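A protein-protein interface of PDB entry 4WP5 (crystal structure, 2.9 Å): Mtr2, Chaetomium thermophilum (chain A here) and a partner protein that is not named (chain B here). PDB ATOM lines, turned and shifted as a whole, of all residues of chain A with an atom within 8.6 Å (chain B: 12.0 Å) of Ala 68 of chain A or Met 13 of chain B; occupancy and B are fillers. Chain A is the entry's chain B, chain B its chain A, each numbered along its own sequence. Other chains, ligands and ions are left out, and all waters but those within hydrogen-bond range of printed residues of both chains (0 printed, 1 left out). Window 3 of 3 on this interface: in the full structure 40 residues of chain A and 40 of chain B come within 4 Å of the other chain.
The backbone NH (N) of Leu 17 of chain B is in hydrogen-bond range of the side-chain amide oxygen (OE1) of Gln 66 of chain A. The backbone carbonyl oxygen (O) of Gln 66 of chain A lies close to the backbone carbonyl oxygen (O) of Thr 15 of chain B, at 3.4 Å.
The backbone carbonyl oxygen (O) of Phe 133 of chain A sits at hydrogen-bond distance from the backbone NH (N) of Val 144 of chain A (2.9 Å).
Met 62 of chain A touches Leu 17 of chain B. CA of Pro 16 of chain B touches OE1 of Gln 66 of chain A, at 3.6 Å. Ala 68 of chain A touches Met 13 of chain B. CZ of Phe 133 of chain A touches CB of Pro 16 of chain B (3.6 Å).
Lys 64 of chain A touches none of the printed residues of chain B. Ala 68 of chain A touches one residue of chain B. Of chain A, only Ala 68 (3.0 Å) comes within 4 Å of Met 13 of chain B. Printed residues of chain A within 4 Å of Thr 15 of chain B: Gln 66 (3.4 Å). Of the printed residues of chain A, Pro 16 of chain B touches Gln 66 (3.6 Å) and Phe 133 (3.6 Å). Of the printed residues of chain A, Leu 17 of chain B touches Met 62 and Gln 66. The nearest residue of chain B that does not touch Ala 68 of chain A is Pro 14 of chain B (4.1 Å).
Hydrophobic or aromatic side chains of chain B within 4 Å of the printed part of chain A: Met 13, Pro 16 and Leu 17. Printed residues of chain A that touch a printed residue of chain B: Met 62, Gln 66, Ala 68 and Phe 133. Hydrophobic or aromatic side chains of chain A that line the printed part of chain B: Met 62, Ala 68 and Phe 133. Among the printed residues, 6 pairs touch across the chains. Among the printed residues, no Asp or Glu carboxylate lies within 4 Å of a Lys or Arg side-chain nitrogen of the other chain.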
ATOM      1  N   ASN A  22      23.652  -1.269  34.428  1.00  0.00           N
ATOM      2  CA  ASN A  22      22.663  -0.219  34.199  1.00  0.00           C
ATOM      3  C   ASN A  22      23.068   1.095  34.862  1.00  0.00           C
ATOM      4  O   ASN A  22      22.246   1.764  35.491  1.00  0.00           O
ATOM      5  CB  ASN A  22      21.285  -0.658  34.703  1.00  0.00           C
ATOM      6  CG  ASN A  22      20.772  -1.898  33.993  1.00  0.00           C
ATOM      7  OD1 ASN A  22      21.551  -2.722  33.515  1.00  0.00           O
ATOM      8  ND2 ASN A  22      19.452  -2.032  33.917  1.00  0.00           N
ATOM      9  N   THR A  61      20.754   7.279  27.437  1.00  0.00           N
ATOM     10  CA  THR A  61      19.310   7.130  27.317  1.00  0.00           C
ATOM     11  C   THR A  61      18.975   6.032  26.310  1.00  0.00           C
ATOM     12  O   THR A  61      18.094   5.208  26.552  1.00  0.00           O
ATOM     13  CB  THR A  61      18.635   8.442  26.881  1.00  0.00           C
ATOM     14  OG1 THR A  61      19.027   9.501  27.762  1.00  0.00           O
ATOM     15  CG2 THR A  61      17.119   8.298  26.905  1.00  0.00           C
ATOM     16  N   MET A  62      19.680   6.029  25.182  1.00  0.00           N
ATOM     17  CA  MET A  62      19.503   4.993  24.169  1.00  0.00           C
ATOM     18  C   MET A  62      19.747   3.611  24.762  1.00  0.00           C
ATOM     19  O   MET A  62      19.031   2.657  24.453  1.00  0.00           O
ATOM     20  CB  MET A  62      20.446   5.226  22.987  1.00  0.00           C
ATOM     21  CG  MET A  62      20.094   6.432  22.132  1.00  0.00           C
ATOM     22  SD  MET A  62      21.354   6.810  20.898  1.00  0.00           S
ATOM     23  CE  MET A  62      21.248   5.368  19.840  1.00  0.00           C
ATOM     24  N   LEU A  63      20.765   3.506  25.611  1.00  0.00           N
ATOM     25  CA  LEU A  63      21.062   2.257  26.303  1.00  0.00           C
ATOM     26  C   LEU A  63      19.893   1.836  27.190  1.00  0.00           C
ATOM     27  O   LEU A  63      19.644   0.646  27.376  1.00  0.00           O
ATOM     28  CB  LEU A  63      22.339   2.398  27.134  1.00  0.00           C
ATOM     29  CG  LEU A  63      23.648   2.328  26.343  1.00  0.00           C
ATOM     30  CD1 LEU A  63      24.828   2.739  27.210  1.00  0.00           C
ATOM     31  CD2 LEU A  63      23.859   0.928  25.785  1.00  0.00           C
ATOM     32  N   LYS A  64      19.178   2.819  27.731  1.00  0.00           N
ATOM     33  CA  LYS A  64      17.981   2.546  28.520  1.00  0.00           C
ATOM     34  C   LYS A  64      16.820   2.152  27.611  1.00  0.00           C
ATOM     35  O   LYS A  64      16.027   1.275  27.951  1.00  0.00           O
ATOM     36  CB  LYS A  64      17.601   3.762  29.369  1.00  0.00           C
ATOM     37  CG  LYS A  64      18.174   3.741  30.776  1.00  0.00           C
ATOM     38  CD  LYS A  64      17.174   3.177  31.775  1.00  0.00           C
ATOM     39  CE  LYS A  64      17.873   2.665  33.022  1.00  0.00           C
ATOM     40  NZ  LYS A  64      16.924   2.336  34.120  1.00  0.00           N
ATOM     41  N   GLU A  65      16.728   2.805  26.455  1.00  0.00           N
ATOM     42  CA  GLU A  65      15.694   2.490  25.473  1.00  0.00           C
ATOM     43  C   GLU A  65      15.816   1.046  25.002  1.00  0.00           C
ATOM     44  O   GLU A  65      14.816   0.342  24.862  1.00  0.00           O
ATOM     45  CB  GLU A  65      15.783   3.437  24.273  1.00  0.00           C
ATOM     46  CG  GLU A  65      15.466   4.892  24.591  1.00  0.00           C
ATOM     47  CD  GLU A  65      13.995   5.128  24.872  1.00  0.00           C
ATOM     48  OE1 GLU A  65      13.148   4.517  24.185  1.00  0.00           O
ATOM     49  OE2 GLU A  65      13.684   5.925  25.783  1.00  0.00           O
ATOM     50  N   GLN A  66      17.050   0.612  24.759  1.00  0.00           N
ATOM     51  CA  GLN A  66      17.314  -0.745  24.294  1.00  0.00           C
ATOM     52  C   GLN A  66      16.898  -1.782  25.332  1.00  0.00           C
ATOM     53  O   GLN A  66      16.463  -2.880  24.983  1.00  0.00           O
ATOM     54  CB  GLN A  66      18.797  -0.912  23.954  1.00  0.00           C
ATOM     55  CG  GLN A  66      19.166  -2.306  23.466  1.00  0.00           C
ATOM     56  CD  GLN A  66      20.566  -2.380  22.884  1.00  0.00           C
ATOM     57  OE1 GLN A  66      20.829  -3.166  21.975  1.00  0.00           O
ATOM     58  NE2 GLN A  66      21.475  -1.564  23.409  1.00  0.00           N
ATOM     59  N   ARG A  67      17.030  -1.428  26.607  1.00  0.00           N
ATOM     60  CA  ARG A  67      16.672  -2.334  27.692  1.00  0.00           C
ATOM     61  C   ARG A  67      15.159  -2.436  27.864  1.00  0.00           C
ATOM     62  O   ARG A  67      14.674  -3.276  28.622  1.00  0.00           O
ATOM     63  CB  ARG A  67      17.314  -1.877  29.007  1.00  0.00           C
ATOM     64  CG  ARG A  67      18.423  -2.792  29.518  1.00  0.00           C
ATOM     65  CD  ARG A  67      19.745  -2.055  29.648  1.00  0.00           C
ATOM     66  NE  ARG A  67      19.710  -1.043  30.698  1.00  0.00           N
ATOM     67  CZ  ARG A  67      20.704  -0.199  30.958  1.00  0.00           C
ATOM     68  NH1 ARG A  67      21.820  -0.235  30.242  1.00  0.00           N
ATOM     69  NH2 ARG A  67      20.580   0.688  31.934  1.00  0.00           N
ATOM     70  N   ALA A  68      14.421  -1.583  27.157  1.00  0.00           N
ATOM     71  CA  ALA A  68      12.962  -1.581  27.214  1.00  0.00           C
ATOM     72  C   ALA A  68      12.464  -1.392  28.645  1.00  0.00           C
ATOM     73  O   ALA A  68      11.917  -0.345  28.988  1.00  0.00           O
ATOM     74  CB  ALA A  68      12.407  -2.871  26.628  1.00  0.00           C
ATOM     75  N   PRO A  84      17.530  -8.642  30.393  1.00  0.00           N
ATOM     76  CA  PRO A  84      17.085  -8.077  29.112  1.00  0.00           C
ATOM     77  C   PRO A  84      18.214  -7.897  28.099  1.00  0.00           C
ATOM     78  O   PRO A  84      18.062  -8.309  26.950  1.00  0.00           O
ATOM     79  CB  PRO A  84      16.495  -6.721  29.512  1.00  0.00           C
ATOM     80  CG  PRO A  84      17.161  -6.377  30.791  1.00  0.00           C
ATOM     81  CD  PRO A  84      17.367  -7.679  31.498  1.00  0.00           C
ATOM     82  N   VAL A  85      19.320  -7.286  28.518  1.00  0.00           N
ATOM     83  CA  VAL A  85      20.451  -7.044  27.624  1.00  0.00           C
ATOM     84  C   VAL A  85      21.774  -7.199  28.365  1.00  0.00           C
ATOM     85  O   VAL A  85      21.958  -6.629  29.439  1.00  0.00           O
ATOM     86  CB  VAL A  85      20.388  -5.633  27.000  1.00  0.00           C
ATOM     87  CG1 VAL A  85      21.522  -5.442  26.002  1.00  0.00           C
ATOM     88  CG2 VAL A  85      19.036  -5.396  26.336  1.00  0.00           C
ATOM     89  N   PHE A 133      20.307 -10.775  23.976  1.00  0.00           N
ATOM     90  CA  PHE A 133      19.022 -10.200  24.364  1.00  0.00           C
ATOM     91  C   PHE A 133      18.109 -11.262  24.969  1.00  0.00           C
ATOM     92  O   PHE A 133      17.859 -12.298  24.354  1.00  0.00           O
ATOM     93  CB  PHE A 133      18.339  -9.555  23.159  1.00  0.00           C
ATOM     94  CG  PHE A 133      19.082  -8.376  22.602  1.00  0.00           C
ATOM     95  CD1 PHE A 133      20.075  -8.551  21.654  1.00  0.00           C
ATOM     96  CD2 PHE A 133      18.786  -7.092  23.025  1.00  0.00           C
ATOM     97  CE1 PHE A 133      20.758  -7.470  21.138  1.00  0.00           C
ATOM     98  CE2 PHE A 133      19.468  -6.005  22.513  1.00  0.00           C
ATOM     99  CZ  PHE A 133      20.455  -6.195  21.569  1.00  0.00           C
ATOM    100  N   GLY A 134      17.617 -10.994  26.175  1.00  0.00           N
ATOM    101  CA  GLY A 134      16.718 -11.906  26.858  1.00  0.00           C
ATOM    102  C   GLY A 134      17.330 -13.276  27.075  1.00  0.00           C
ATOM    103  O   GLY A 134      16.794 -14.284  26.612  1.00  0.00           O
ATOM    104  N   VAL A 144      16.965 -14.789  23.190  1.00  0.00           N
ATOM    105  CA  VAL A 144      15.945 -14.361  22.244  1.00  0.00           C
ATOM    106  C   VAL A 144      16.607 -14.046  20.908  1.00  0.00           C
ATOM    107  O   VAL A 144      16.283 -14.650  19.883  1.00  0.00           O
ATOM    108  CB  VAL A 144      15.175 -13.122  22.746  1.00  0.00           C
ATOM    109  CG1 VAL A 144      14.119 -12.705  21.733  1.00  0.00           C
ATOM    110  CG2 VAL A 144      14.541 -13.399  24.103  1.00  0.00           C
ATOM    111  N   MET B  13      10.215  -7.862  26.527  1.00  0.00           N
ATOM    112  CA  MET B  13      10.060  -6.622  25.777  1.00  0.00           C
ATOM    113  C   MET B  13      11.360  -6.058  25.171  1.00  0.00           C
ATOM    114  O   MET B  13      11.375  -4.908  24.733  1.00  0.00           O
ATOM    115  CB  MET B  13       9.433  -5.560  26.687  1.00  0.00           C
ATOM    116  CG  MET B  13      10.051  -5.504  28.076  1.00  0.00           C
ATOM    117  SD  MET B  13       9.911  -3.885  28.858  1.00  0.00           S
ATOM    118  CE  MET B  13       8.159  -3.560  28.675  1.00  0.00           C
ATOM    119  N   PRO B  14      12.446  -6.855  25.118  1.00  0.00           N
ATOM    120  CA  PRO B  14      13.683  -6.219  24.643  1.00  0.00           C
ATOM    121  C   PRO B  14      13.661  -5.880  23.153  1.00  0.00           C
ATOM    122  O   PRO B  14      13.002  -6.568  22.373  1.00  0.00           O
ATOM    123  CB  PRO B  14      14.747  -7.277  24.941  1.00  0.00           C
ATOM    124  CG  PRO B  14      14.023  -8.562  24.826  1.00  0.00           C
ATOM    125  CD  PRO B  14      12.639  -8.298  25.351  1.00  0.00           C
ATOM    126  N   THR B  15      14.379  -4.825  22.777  1.00  0.00           N
ATOM    127  CA  THR B  15      14.453  -4.386  21.386  1.00  0.00           C
ATOM    128  C   THR B  15      15.845  -3.823  21.080  1.00  0.00           C
ATOM    129  O   THR B  15      16.215  -2.779  21.617  1.00  0.00           O
ATOM    130  CB  THR B  15      13.394  -3.311  21.073  1.00  0.00           C
ATOM    131  OG1 THR B  15      13.540  -2.211  21.981  1.00  0.00           O
ATOM    132  CG2 THR B  15      11.991  -3.886  21.197  1.00  0.00           C
ATOM    133  N   PRO B  16      16.622  -4.511  20.221  1.00  0.00           N
ATOM    134  CA  PRO B  16      17.969  -4.030  19.883  1.00  0.00           C
ATOM    135  C   PRO B  16      17.981  -2.617  19.306  1.00  0.00           C
ATOM    136  O   PRO B  16      16.951  -2.131  18.840  1.00  0.00           O
ATOM    137  CB  PRO B  16      18.452  -5.042  18.838  1.00  0.00           C
ATOM    138  CG  PRO B  16      17.672  -6.273  19.110  1.00  0.00           C
ATOM    139  CD  PRO B  16      16.330  -5.806  19.578  1.00  0.00           C
ATOM    140  N   LEU B  17      19.144  -1.971  19.341  1.00  0.00           N
ATOM    141  CA  LEU B  17      19.286  -0.610  18.832  1.00  0.00           C
ATOM    142  C   LEU B  17      19.016  -0.547  17.330  1.00  0.00           C
ATOM    143  O   LEU B  17      19.190  -1.540  16.625  1.00  0.00           O
ATOM    144  CB  LEU B  17      20.688  -0.069  19.130  1.00  0.00           C
ATOM    145  CG  LEU B  17      20.953   0.425  20.554  1.00  0.00           C
ATOM    146  CD1 LEU B  17      22.441   0.649  20.766  1.00  0.00           C
ATOM    147  CD2 LEU B  17      20.170   1.702  20.835  1.00  0.00           C
ATOM    148  N   PRO B  18      18.591   0.628  16.837  1.00  0.00           N
ATOM    149  CA  PRO B  18      18.327   0.798  15.403  1.00  0.00           C
ATOM    150  C   PRO B  18      19.610   0.806  14.577  1.00  0.00           C
ATOM    151  O   PRO B  18      20.564   1.500  14.933  1.00  0.00           O
ATOM    152  CB  PRO B  18      17.621   2.153  15.335  1.00  0.00           C
ATOM    153  CG  PRO B  18      18.112   2.894  16.527  1.00  0.00           C
ATOM    154  CD  PRO B  18      18.324   1.862  17.596  1.00  0.00           C
